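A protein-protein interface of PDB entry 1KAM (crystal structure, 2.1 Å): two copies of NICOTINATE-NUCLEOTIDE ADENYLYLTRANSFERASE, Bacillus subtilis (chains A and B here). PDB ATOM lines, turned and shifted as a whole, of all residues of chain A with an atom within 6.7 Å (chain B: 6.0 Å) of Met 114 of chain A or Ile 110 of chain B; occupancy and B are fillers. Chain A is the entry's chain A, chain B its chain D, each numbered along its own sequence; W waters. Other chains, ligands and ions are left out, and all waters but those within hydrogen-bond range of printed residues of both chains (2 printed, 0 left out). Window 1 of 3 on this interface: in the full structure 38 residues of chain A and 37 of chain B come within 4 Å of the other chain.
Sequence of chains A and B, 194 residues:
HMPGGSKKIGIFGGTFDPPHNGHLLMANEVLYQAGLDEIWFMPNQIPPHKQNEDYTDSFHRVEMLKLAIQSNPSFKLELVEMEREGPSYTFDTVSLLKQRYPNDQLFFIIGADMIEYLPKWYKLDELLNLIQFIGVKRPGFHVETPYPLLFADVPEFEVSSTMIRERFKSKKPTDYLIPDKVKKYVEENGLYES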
ATOM      1  N   PHE A 108      -8.603  11.227 -27.566  1.00  0.00           N
ATOM      2  CA  PHE A 108      -8.375   9.825 -27.238  1.00  0.00           C
ATOM      3  C   PHE A 108      -8.183   9.659 -25.725  1.00  0.00           C
ATOM      4  O   PHE A 108      -7.293  10.272 -25.128  1.00  0.00           O
ATOM      5  CB  PHE A 108      -7.151   9.296 -27.977  1.00  0.00           C
ATOM      6  CG  PHE A 108      -7.107   7.797 -28.059  1.00  0.00           C
ATOM      7  CD1 PHE A 108      -7.936   7.112 -28.946  1.00  0.00           C
ATOM      8  CD2 PHE A 108      -6.267   7.065 -27.225  1.00  0.00           C
ATOM      9  CE1 PHE A 108      -7.927   5.711 -28.999  1.00  0.00           C
ATOM     10  CE2 PHE A 108      -6.252   5.670 -27.270  1.00  0.00           C
ATOM     11  CZ  PHE A 108      -7.082   4.992 -28.158  1.00  0.00           C
ATOM     12  N   ILE A 110      -7.132   7.728 -22.324  1.00  0.00           N
ATOM     13  CA  ILE A 110      -6.189   6.732 -21.811  1.00  0.00           C
ATOM     14  C   ILE A 110      -5.996   7.014 -20.326  1.00  0.00           C
ATOM     15  O   ILE A 110      -6.476   8.032 -19.808  1.00  0.00           O
ATOM     16  CB  ILE A 110      -4.786   6.837 -22.469  1.00  0.00           C
ATOM     17  CG1 ILE A 110      -4.282   8.276 -22.360  1.00  0.00           C
ATOM     18  CG2 ILE A 110      -4.832   6.387 -23.931  1.00  0.00           C
ATOM     19  CD1 ILE A 110      -2.762   8.405 -22.437  1.00  0.00           C
ATOM     20  N   GLY A 111      -5.301   6.111 -19.644  1.00  0.00           N
ATOM     21  CA  GLY A 111      -5.022   6.313 -18.239  1.00  0.00           C
ATOM     22  C   GLY A 111      -3.951   7.385 -18.220  1.00  0.00           C
ATOM     23  O   GLY A 111      -3.050   7.374 -19.060  1.00  0.00           O
ATOM     24  N   ALA A 112      -4.043   8.318 -17.281  1.00  0.00           N
ATOM     25  CA  ALA A 112      -3.069   9.403 -17.208  1.00  0.00           C
ATOM     26  C   ALA A 112      -1.630   8.923 -16.980  1.00  0.00           C
ATOM     27  O   ALA A 112      -0.676   9.636 -17.296  1.00  0.00           O
ATOM     28  CB  ALA A 112      -3.474  10.379 -16.103  1.00  0.00           C
ATOM     29  N   ASP A 113      -1.481   7.721 -16.436  1.00  0.00           N
ATOM     30  CA  ASP A 113      -0.161   7.170 -16.149  1.00  0.00           C
ATOM     31  C   ASP A 113       0.389   6.319 -17.278  1.00  0.00           C
ATOM     32  O   ASP A 113       1.536   5.884 -17.216  1.00  0.00           O
ATOM     33  CB  ASP A 113      -0.217   6.311 -14.881  1.00  0.00           C
ATOM     34  CG  ASP A 113      -1.061   5.062 -15.068  1.00  0.00           C
ATOM     35  OD1 ASP A 113      -2.130   5.153 -15.705  1.00  0.00           O
ATOM     36  OD2 ASP A 113      -0.664   3.988 -14.579  1.00  0.00           O
ATOM     37  N   MET A 114      -0.410   6.079 -18.311  1.00  0.00           N
ATOM     38  CA  MET A 114       0.055   5.227 -19.399  1.00  0.00           C
ATOM     39  C   MET A 114       1.441   5.610 -19.885  1.00  0.00           C
ATOM     40  O   MET A 114       2.303   4.742 -20.044  1.00  0.00           O
ATOM     41  CB  MET A 114      -0.918   5.244 -20.596  1.00  0.00           C
ATOM     42  CG  MET A 114      -0.627   4.133 -21.653  1.00  0.00           C
ATOM     43  SD  MET A 114      -1.799   3.994 -23.039  1.00  0.00           S
ATOM     44  CE  MET A 114      -1.085   5.090 -24.194  1.00  0.00           C
ATOM     45  N   ILE A 115       1.660   6.908 -20.091  1.00  0.00           N
ATOM     46  CA  ILE A 115       2.933   7.395 -20.625  1.00  0.00           C
ATOM     47  C   ILE A 115       3.861   8.108 -19.642  1.00  0.00           C
ATOM     48  O   ILE A 115       4.898   8.646 -20.038  1.00  0.00           O
ATOM     49  CB  ILE A 115       2.678   8.345 -21.808  1.00  0.00           C
ATOM     50  CG1 ILE A 115       1.833   9.539 -21.341  1.00  0.00           C
ATOM     51  CG2 ILE A 115       1.979   7.593 -22.935  1.00  0.00           C
ATOM     52  CD1 ILE A 115       1.622  10.614 -22.394  1.00  0.00           C
ATOM     53  N   GLU A 116       3.491   8.096 -18.366  1.00  0.00           N
ATOM     54  CA  GLU A 116       4.255   8.755 -17.315  1.00  0.00           C
ATOM     55  C   GLU A 116       5.710   8.311 -17.184  1.00  0.00           C
ATOM     56  O   GLU A 116       6.573   9.111 -16.846  1.00  0.00           O
ATOM     57  CB  GLU A 116       3.567   8.535 -15.966  1.00  0.00           C
ATOM     58  CG  GLU A 116       4.080   9.431 -14.848  1.00  0.00           C
ATOM     59  CD  GLU A 116       3.433   9.106 -13.513  1.00  0.00           C
ATOM     60  OE1 GLU A 116       2.252   8.695 -13.523  1.00  0.00           O
ATOM     61  OE2 GLU A 116       4.096   9.270 -12.461  1.00  0.00           O
ATOM     62  N   TYR A 117       5.974   7.041 -17.459  1.00  0.00           N
ATOM     63  CA  TYR A 117       7.317   6.489 -17.313  1.00  0.00           C
ATOM     64  C   TYR A 117       8.131   6.360 -18.598  1.00  0.00           C
ATOM     65  O   TYR A 117       9.249   5.862 -18.571  1.00  0.00           O
ATOM     66  CB  TYR A 117       7.215   5.114 -16.637  1.00  0.00           C
ATOM     67  CG  TYR A 117       6.248   5.120 -15.477  1.00  0.00           C
ATOM     68  CD1 TYR A 117       5.037   4.431 -15.546  1.00  0.00           C
ATOM     69  CD2 TYR A 117       6.511   5.885 -14.335  1.00  0.00           C
ATOM     70  CE1 TYR A 117       4.102   4.510 -14.501  1.00  0.00           C
ATOM     71  CE2 TYR A 117       5.592   5.970 -13.293  1.00  0.00           C
ATOM     72  CZ  TYR A 117       4.393   5.282 -13.385  1.00  0.00           C
ATOM     73  OH  TYR A 117       3.489   5.382 -12.359  1.00  0.00           O
ATOM     74  N   LEU A 118       7.582   6.800 -19.720  1.00  0.00           N
ATOM     75  CA  LEU A 118       8.303   6.695 -20.983  1.00  0.00           C
ATOM     76  C   LEU A 118       9.274   7.849 -21.205  1.00  0.00           C
ATOM     77  O   LEU A 118       9.012   8.971 -20.786  1.00  0.00           O
ATOM     78  CB  LEU A 118       7.309   6.647 -22.149  1.00  0.00           C
ATOM     79  CG  LEU A 118       6.384   5.429 -22.222  1.00  0.00           C
ATOM     80  CD1 LEU A 118       5.339   5.647 -23.296  1.00  0.00           C
ATOM     81  CD2 LEU A 118       7.194   4.172 -22.525  1.00  0.00           C
ATOM     82  N   TRP A 121      10.172  10.022 -26.975  1.00  0.00           N
ATOM     83  CA  TRP A 121       9.948   9.078 -28.068  1.00  0.00           C
ATOM     84  C   TRP A 121       9.106   9.713 -29.173  1.00  0.00           C
ATOM     85  O   TRP A 121       7.954  10.063 -28.943  1.00  0.00           O
ATOM     86  CB  TRP A 121       9.226   7.851 -27.517  1.00  0.00           C
ATOM     87  CG  TRP A 121       9.262   6.671 -28.415  1.00  0.00           C
ATOM     88  CD1 TRP A 121       9.891   6.572 -29.623  1.00  0.00           C
ATOM     89  CD2 TRP A 121       8.700   5.388 -28.146  1.00  0.00           C
ATOM     90  NE1 TRP A 121       9.759   5.300 -30.121  1.00  0.00           N
ATOM     91  CE2 TRP A 121       9.032   4.551 -29.233  1.00  0.00           C
ATOM     92  CE3 TRP A 121       7.948   4.861 -27.088  1.00  0.00           C
ATOM     93  CZ2 TRP A 121       8.641   3.212 -29.293  1.00  0.00           C
ATOM     94  CZ3 TRP A 121       7.558   3.530 -27.147  1.00  0.00           C
ATOM     95  CH2 TRP A 121       7.906   2.719 -28.245  1.00  0.00           C
ATOM     96  N   LEU A 124       5.668   8.277 -30.113  1.00  0.00           N
ATOM     97  CA  LEU A 124       4.612   8.654 -29.190  1.00  0.00           C
ATOM     98  C   LEU A 124       4.203  10.100 -29.490  1.00  0.00           C
ATOM     99  O   LEU A 124       3.015  10.421 -29.546  1.00  0.00           O
ATOM    100  CB  LEU A 124       5.096   8.539 -27.741  1.00  0.00           C
ATOM    101  CG  LEU A 124       4.138   9.135 -26.703  1.00  0.00           C
ATOM    102  CD1 LEU A 124       2.792   8.436 -26.803  1.00  0.00           C
ATOM    103  CD2 LEU A 124       4.707   8.993 -25.309  1.00  0.00           C
ATOM    104  N   LEU A 127       1.881  10.249 -32.285  1.00  0.00           N
ATOM    105  CA  LEU A 127       0.528   9.827 -31.957  1.00  0.00           C
ATOM    106  C   LEU A 127      -0.202  10.933 -31.198  1.00  0.00           C
ATOM    107  O   LEU A 127      -1.393  11.161 -31.410  1.00  0.00           O
ATOM    108  CB  LEU A 127       0.562   8.541 -31.123  1.00  0.00           C
ATOM    109  CG  LEU A 127      -0.786   7.932 -30.727  1.00  0.00           C
ATOM    110  CD1 LEU A 127      -1.656   7.758 -31.957  1.00  0.00           C
ATOM    111  CD2 LEU A 127      -0.558   6.586 -30.044  1.00  0.00           C
ATOM    112  N   PHE A 133      -4.999  13.817 -26.610  1.00  0.00           N
ATOM    113  CA  PHE A 133      -5.178  12.774 -25.609  1.00  0.00           C
ATOM    114  C   PHE A 133      -5.735  13.323 -24.297  1.00  0.00           C
ATOM    115  O   PHE A 133      -5.400  14.435 -23.882  1.00  0.00           O
ATOM    116  CB  PHE A 133      -3.839  12.079 -25.321  1.00  0.00           C
ATOM    117  CG  PHE A 133      -3.525  10.947 -26.258  1.00  0.00           C
ATOM    118  CD1 PHE A 133      -3.566  11.130 -27.636  1.00  0.00           C
ATOM    119  CD2 PHE A 133      -3.196   9.693 -25.756  1.00  0.00           C
ATOM    120  CE1 PHE A 133      -3.285  10.076 -28.505  1.00  0.00           C
ATOM    121  CE2 PHE A 133      -2.913   8.632 -26.613  1.00  0.00           C
ATOM    122  CZ  PHE A 133      -2.959   8.826 -27.993  1.00  0.00           C
ATOM    123  N   PHE B 108      10.452  -1.034 -21.732  1.00  0.00           N
ATOM    124  CA  PHE B 108       9.907   0.264 -21.348  1.00  0.00           C
ATOM    125  C   PHE B 108       8.703   0.042 -20.443  1.00  0.00           C
ATOM    126  O   PHE B 108       7.979  -0.943 -20.575  1.00  0.00           O
ATOM    127  CB  PHE B 108       9.545   1.082 -22.590  1.00  0.00           C
ATOM    128  CG  PHE B 108      10.743   1.472 -23.416  1.00  0.00           C
ATOM    129  CD1 PHE B 108      11.257   0.609 -24.379  1.00  0.00           C
ATOM    130  CD2 PHE B 108      11.383   2.685 -23.201  1.00  0.00           C
ATOM    131  CE1 PHE B 108      12.394   0.948 -25.114  1.00  0.00           C
ATOM    132  CE2 PHE B 108      12.519   3.033 -23.930  1.00  0.00           C
ATOM    133  CZ  PHE B 108      13.024   2.162 -24.888  1.00  0.00           C
ATOM    134  N   ILE B 109       8.500   0.965 -19.513  1.00  0.00           N
ATOM    135  CA  ILE B 109       7.436   0.831 -18.532  1.00  0.00           C
ATOM    136  C   ILE B 109       6.178   1.625 -18.858  1.00  0.00           C
ATOM    137  O   ILE B 109       6.235   2.835 -19.076  1.00  0.00           O
ATOM    138  CB  ILE B 109       7.983   1.228 -17.151  1.00  0.00           C
ATOM    139  CG1 ILE B 109       9.222   0.369 -16.843  1.00  0.00           C
ATOM    140  CG2 ILE B 109       6.890   1.084 -16.089  1.00  0.00           C
ATOM    141  CD1 ILE B 109      10.073   0.857 -15.679  1.00  0.00           C
ATOM    142  N   ILE B 110       5.046   0.920 -18.885  1.00  0.00           N
ATOM    143  CA  ILE B 110       3.754   1.511 -19.198  1.00  0.00           C
ATOM    144  C   ILE B 110       2.828   1.520 -17.971  1.00  0.00           C
ATOM    145  O   ILE B 110       2.607   0.489 -17.332  1.00  0.00           O
ATOM    146  CB  ILE B 110       3.043   0.718 -20.339  1.00  0.00           C
ATOM    147  CG1 ILE B 110       3.950   0.618 -21.568  1.00  0.00           C
ATOM    148  CG2 ILE B 110       1.729   1.406 -20.719  1.00  0.00           C
ATOM    149  CD1 ILE B 110       4.298   1.964 -22.209  1.00  0.00           C
ATOM    150  N   GLY B 111       2.293   2.686 -17.641  1.00  0.00           N
ATOM    151  CA  GLY B 111       1.384   2.765 -16.516  1.00  0.00           C
ATOM    152  C   GLY B 111       0.042   2.194 -16.941  1.00  0.00           C
ATOM    153  O   GLY B 111      -0.424   2.467 -18.044  1.00  0.00           O
ATOM    154  N   ALA B 112      -0.568   1.383 -16.082  1.00  0.00           N
ATOM    155  CA  ALA B 112      -1.875   0.786 -16.364  1.00  0.00           C
ATOM    156  C   ALA B 112      -2.604   0.674 -15.038  1.00  0.00           C
ATOM    157  O   ALA B 112      -3.220  -0.342 -14.744  1.00  0.00           O
ATOM    158  CB  ALA B 112      -1.708  -0.607 -16.978  1.00  0.00           C
ATOM    159  N   LEU B 118      -5.785  -1.156 -21.872  1.00  0.00           N
ATOM    160  CA  LEU B 118      -4.560  -0.580 -22.407  1.00  0.00           C
ATOM    161  C   LEU B 118      -4.621  -0.796 -23.922  1.00  0.00           C
ATOM    162  O   LEU B 118      -4.573  -1.932 -24.395  1.00  0.00           O
ATOM    163  CB  LEU B 118      -3.349  -1.300 -21.810  1.00  0.00           C
ATOM    164  CG  LEU B 118      -1.984  -0.619 -21.845  1.00  0.00           C
ATOM    165  CD1 LEU B 118      -0.963  -1.586 -21.257  1.00  0.00           C
ATOM    166  CD2 LEU B 118      -1.604  -0.246 -23.265  1.00  0.00           C
ATOM    167  N   PRO B 119      -4.732   0.299 -24.700  1.00  0.00           N
ATOM    168  CA  PRO B 119      -4.809   0.246 -26.166  1.00  0.00           C
ATOM    169  C   PRO B 119      -3.545  -0.230 -26.873  1.00  0.00           C
ATOM    170  O   PRO B 119      -2.442  -0.154 -26.330  1.00  0.00           O
ATOM    171  CB  PRO B 119      -5.146   1.684 -26.539  1.00  0.00           C
ATOM    172  CG  PRO B 119      -4.356   2.460 -25.511  1.00  0.00           C
ATOM    173  CD  PRO B 119      -4.662   1.698 -24.232  1.00  0.00           C
ATOM    174  N   TRP B 121      -1.546   0.990 -28.898  1.00  0.00           N
ATOM    175  CA  TRP B 121      -1.051   2.251 -29.443  1.00  0.00           C
ATOM    176  C   TRP B 121       0.304   2.173 -30.136  1.00  0.00           C
ATOM    177  O   TRP B 121       0.675   3.092 -30.853  1.00  0.00           O
ATOM    178  CB  TRP B 121      -0.952   3.304 -28.340  1.00  0.00           C
ATOM    179  CG  TRP B 121       0.031   2.942 -27.265  1.00  0.00           C
ATOM    180  CD1 TRP B 121      -0.182   2.108 -26.204  1.00  0.00           C
ATOM    181  CD2 TRP B 121       1.383   3.397 -27.149  1.00  0.00           C
ATOM    182  NE1 TRP B 121       0.951   2.019 -25.433  1.00  0.00           N
ATOM    183  CE2 TRP B 121       1.927   2.802 -25.990  1.00  0.00           C
ATOM    184  CE3 TRP B 121       2.188   4.254 -27.910  1.00  0.00           C
ATOM    185  CZ2 TRP B 121       3.242   3.036 -25.574  1.00  0.00           C
ATOM    186  CZ3 TRP B 121       3.496   4.484 -27.494  1.00  0.00           C
ATOM    187  CH2 TRP B 121       4.007   3.877 -26.337  1.00  0.00           C
ATOM    188  N   PHE B 133       7.702  -4.050 -23.523  1.00  0.00           N
ATOM    189  CA  PHE B 133       7.057  -3.213 -22.538  1.00  0.00           C
ATOM    190  C   PHE B 133       6.690  -4.030 -21.325  1.00  0.00           C
ATOM    191  O   PHE B 133       6.587  -5.253 -21.404  1.00  0.00           O
ATOM    192  CB  PHE B 133       5.808  -2.581 -23.148  1.00  0.00           C
ATOM    193  CG  PHE B 133       6.103  -1.660 -24.297  1.00  0.00           C
ATOM    194  CD1 PHE B 133       6.612  -0.383 -24.071  1.00  0.00           C
ATOM    195  CD2 PHE B 133       5.906  -2.079 -25.609  1.00  0.00           C
ATOM    196  CE1 PHE B 133       6.921   0.465 -25.135  1.00  0.00           C
ATOM    197  CE2 PHE B 133       6.212  -1.239 -26.683  1.00  0.00           C
ATOM    198  CZ  PHE B 133       6.721   0.037 -26.442  1.00  0.00           C
ATOM    199  N   ILE B 134       6.518  -3.340 -20.203  1.00  0.00           N
ATOM    200  CA  ILE B 134       6.133  -3.954 -18.942  1.00  0.00           C
ATOM    201  C   ILE B 134       5.096  -3.033 -18.333  1.00  0.00           C
ATOM    202  O   ILE B 134       5.309  -1.823 -18.248  1.00  0.00           O
ATOM    203  CB  ILE B 134       7.321  -4.059 -17.964  1.00  0.00           C
ATOM    204  CG1 ILE B 134       8.375  -5.014 -18.524  1.00  0.00           C
ATOM    205  CG2 ILE B 134       6.830  -4.545 -16.603  1.00  0.00           C
ATOM    206  CD1 ILE B 134       9.621  -5.110 -17.677  1.00  0.00           C
ATOM    207  N   GLY B 135       3.965  -3.589 -17.926  1.00  0.00           N
ATOM    208  CA  GLY B 135       2.944  -2.757 -17.323  1.00  0.00           C
ATOM    209  C   GLY B 135       3.064  -2.729 -15.809  1.00  0.00           C
ATOM    210  O   GLY B 135       3.488  -3.712 -15.202  1.00  0.00           O
ATOM    211  N   VAL B 136       2.730  -1.596 -15.197  1.00  0.00           N
ATOM    212  CA  VAL B 136       2.763  -1.496 -13.746  1.00  0.00           C
ATOM    213  C   VAL B 136       1.362  -1.139 -13.272  1.00  0.00           C
ATOM    214  O   VAL B 136       0.729  -0.222 -13.796  1.00  0.00           O
ATOM    215  CB  VAL B 136       3.767  -0.425 -13.239  1.00  0.00           C
ATOM    216  CG1 VAL B 136       5.180  -0.947 -13.373  1.00  0.00           C
ATOM    217  CG2 VAL B 136       3.604   0.871 -14.008  1.00  0.00           C
ATOM    218  N   LYS B 137       0.874  -1.883 -12.290  1.00  0.00           N
ATOM    219  CA  LYS B 137      -0.458  -1.656 -11.747  1.00  0.00           C
ATOM    220  C   LYS B 137      -0.493  -2.192 -10.328  1.00  0.00           C
ATOM    221  O   LYS B 137       0.366  -2.974  -9.941  1.00  0.00           O
ATOM    222  CB  LYS B 137      -1.503  -2.388 -12.600  1.00  0.00           C
ATOM    223  CG  LYS B 137      -1.318  -3.909 -12.624  1.00  0.00           C
ATOM    224  CD  LYS B 137      -2.379  -4.604 -13.466  1.00  0.00           C
ATOM    225  CE  LYS B 137      -2.241  -6.126 -13.394  1.00  0.00           C
ATOM    226  NZ  LYS B 137      -2.471  -6.633 -11.999  1.00  0.00           N
ATOM    227  N   LEU B 149       1.315  -8.729 -22.783  1.00  0.00           N
ATOM    228  CA  LEU B 149       2.169  -8.015 -21.834  1.00  0.00           C
ATOM    229  C   LEU B 149       2.347  -8.547 -20.411  1.00  0.00           C
ATOM    230  O   LEU B 149       1.404  -9.020 -19.778  1.00  0.00           O
ATOM    231  CB  LEU B 149       1.670  -6.565 -21.762  1.00  0.00           C
ATOM    232  CG  LEU B 149       2.374  -5.540 -20.878  1.00  0.00           C
ATOM    233  CD1 LEU B 149       3.794  -5.356 -21.363  1.00  0.00           C
ATOM    234  CD2 LEU B 149       1.616  -4.222 -20.934  1.00  0.00           C
ATOM    235  N   PHE B 151       2.934  -7.869 -16.533  1.00  0.00           N
ATOM    236  CA  PHE B 151       2.639  -6.785 -15.610  1.00  0.00           C
ATOM    237  C   PHE B 151       3.375  -6.974 -14.287  1.00  0.00           C
ATOM    238  O   PHE B 151       3.635  -8.097 -13.855  1.00  0.00           O
ATOM    239  CB  PHE B 151       1.132  -6.689 -15.325  1.00  0.00           C
ATOM    240  CG  PHE B 151       0.307  -6.205 -16.494  1.00  0.00           C
ATOM    241  CD1 PHE B 151      -0.157  -7.098 -17.457  1.00  0.00           C
ATOM    242  CD2 PHE B 151      -0.018  -4.857 -16.621  1.00  0.00           C
ATOM    243  CE1 PHE B 151      -0.942  -6.656 -18.528  1.00  0.00           C
ATOM    244  CE2 PHE B 151      -0.801  -4.402 -17.691  1.00  0.00           C
ATOM    245  CZ  PHE B 151      -1.264  -5.305 -18.644  1.00  0.00           C
HETATM  246  O   HOH W   1       4.761   4.893 -18.990  1.00  0.00           O
HETATM  247  O   HOH W   2       9.944   3.396 -19.808  1.00  0.00           O
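The backbone NH (N) of Gly 111 of chain B lies close to the backbone carbonyl oxygen (O) of Asp 113 of chain A, at 3.3 Å. OD2 of Asp 113 of chain A is in hydrogen-bond range of N of Ala 112 of chain B. The backbone NH of Gly 111 of chain B lies within hydrogen-bond range of the backbone carbonyl oxygen of Met 114 of chain A (3.2 Å).
The backbone carbonyl oxygen (O) of Phe 108 of chain B sits at hydrogen-bond distance from the backbone NH (N) of Ile 134 of chain B, at 2.8 Å. The backbone NH of Ile 110 of chain B is in hydrogen-bond range of the backbone carbonyl oxygen of Ile 134 of chain B. The backbone carbonyl oxygen (O) of Ile 110 of chain B sits at hydrogen-bond distance from the backbone NH (N) of Val 136 of chain B (3.0 Å). N of Ala 112 of chain B sits at hydrogen-bond distance from O of Val 136 of chain B (3.1 Å).
O of Met 114 of chain A touches CG2 of Ile 110 of chain B, 3.5 Å away. SD of Met 114 of chain A touches CD of Pro 119 of chain B (3.9 Å). Met 114 of chain A touches Trp 121 of chain B. Tyr 117 of chain A touches Ile 109 of chain B (CB to O, 3.5 Å). Gly 111 of chain B touches Tyr 117 of chain A (CA to CE1, 3.8 Å). Tyr 117 of chain A touches Val 136 of chain B. Phe 108 of chain B touches Leu 118 of chain A. Trp 121 of chain B touches Trp 121 of chain A (CH2 to CZ3, 3.7 Å). Trp 121 of chain A touches Phe 133 of chain B. Leu 127 of chain A touches Trp 121 of chain B (CD2 to CB, 3.7 Å).
Of the printed residues of chain B, Asp 113 of chain A touches Gly 111 (3.0 Å) and Ala 112 (3.0 Å). Met 114 of chain A touches four residues of chain B. Of the printed residues of chain B, Leu 118 of chain A touches Phe 108, Ile 109, Ile 110 and Trp 121. Printed residues of chain B within 4 Å of Trp 121 of chain A: Trp 121 (3.7 Å) and Phe 133 (3.4 Å). Printed residues of chain B within 4 Å of Leu 127 of chain A: Trp 121. Of chain A, only Met 114 and Leu 118 come within 4 Å of Ile 110 of chain B. Printed residues of chain A within 4 Å of Gly 111 of chain B: Asp 113 (3.0 Å), Met 114 (3.1 Å) and Tyr 117 (3.8 Å). Leu 118 of chain B touches none of the printed residues of chain A. Ile 134 of chain B touches none of the printed residues of chain A. The nearest residue of chain B that does not touch Met 114 of chain A is Leu 118 of chain B (4.3 Å). The nearest residue of chain A that does not touch Ile 110 of chain B is Tyr 117 of chain A (4.4 Å).
Printed residues of chain B that touch a printed residue of chain A: Phe 108, Ile 109, Ile 110, Gly 111, Ala 112, Pro 119, Trp 121, Phe 133 and Val 136. Hydrophobic or aromatic side chains of chain A that line the printed part of chain B: Met 114, Tyr 117, Leu 118, Trp 121 and Leu 127. Among the printed residues, no Asp or Glu carboxylate lies within 4 Å of a Lys or Arg side-chain nitrogen of the other chain.
Leu 118 of chain A touches Phe 108 of chain B, but with the chains exchanged Phe 108 of chain A does not touch Leu 118 of chain B (7.5 Å). Leu 118 of chain A touches Ile 110 of chain B, but with the chains exchanged Ile 110 of chain A does not touch Leu 118 of chain B (7.1 Å). Trp 121 of chain A touches its own counterpart, Trp 121 of chain B. Trp 121 of chain A touches Phe 133 of chain B, but with the chains exchanged Phe 133 of chain A does not touch Trp 121 of chain B (5.9 Å). Of the 16 pairs that touch across the chains among the printed residues, 1 has its exchanged pair printed and touching as well.
Water W1 lies within hydrogen-bond range of the backbone carbonyl oxygen of Ile 109 of chain B, the backbone carbonyl oxygen of Met 114 of chain A, the backbone NH of Tyr 117 of chain A and the backbone NH of Leu 118 of chain A. Water W2 bridges N of Ile 109 of chain B and O of Tyr 117 of chain A.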
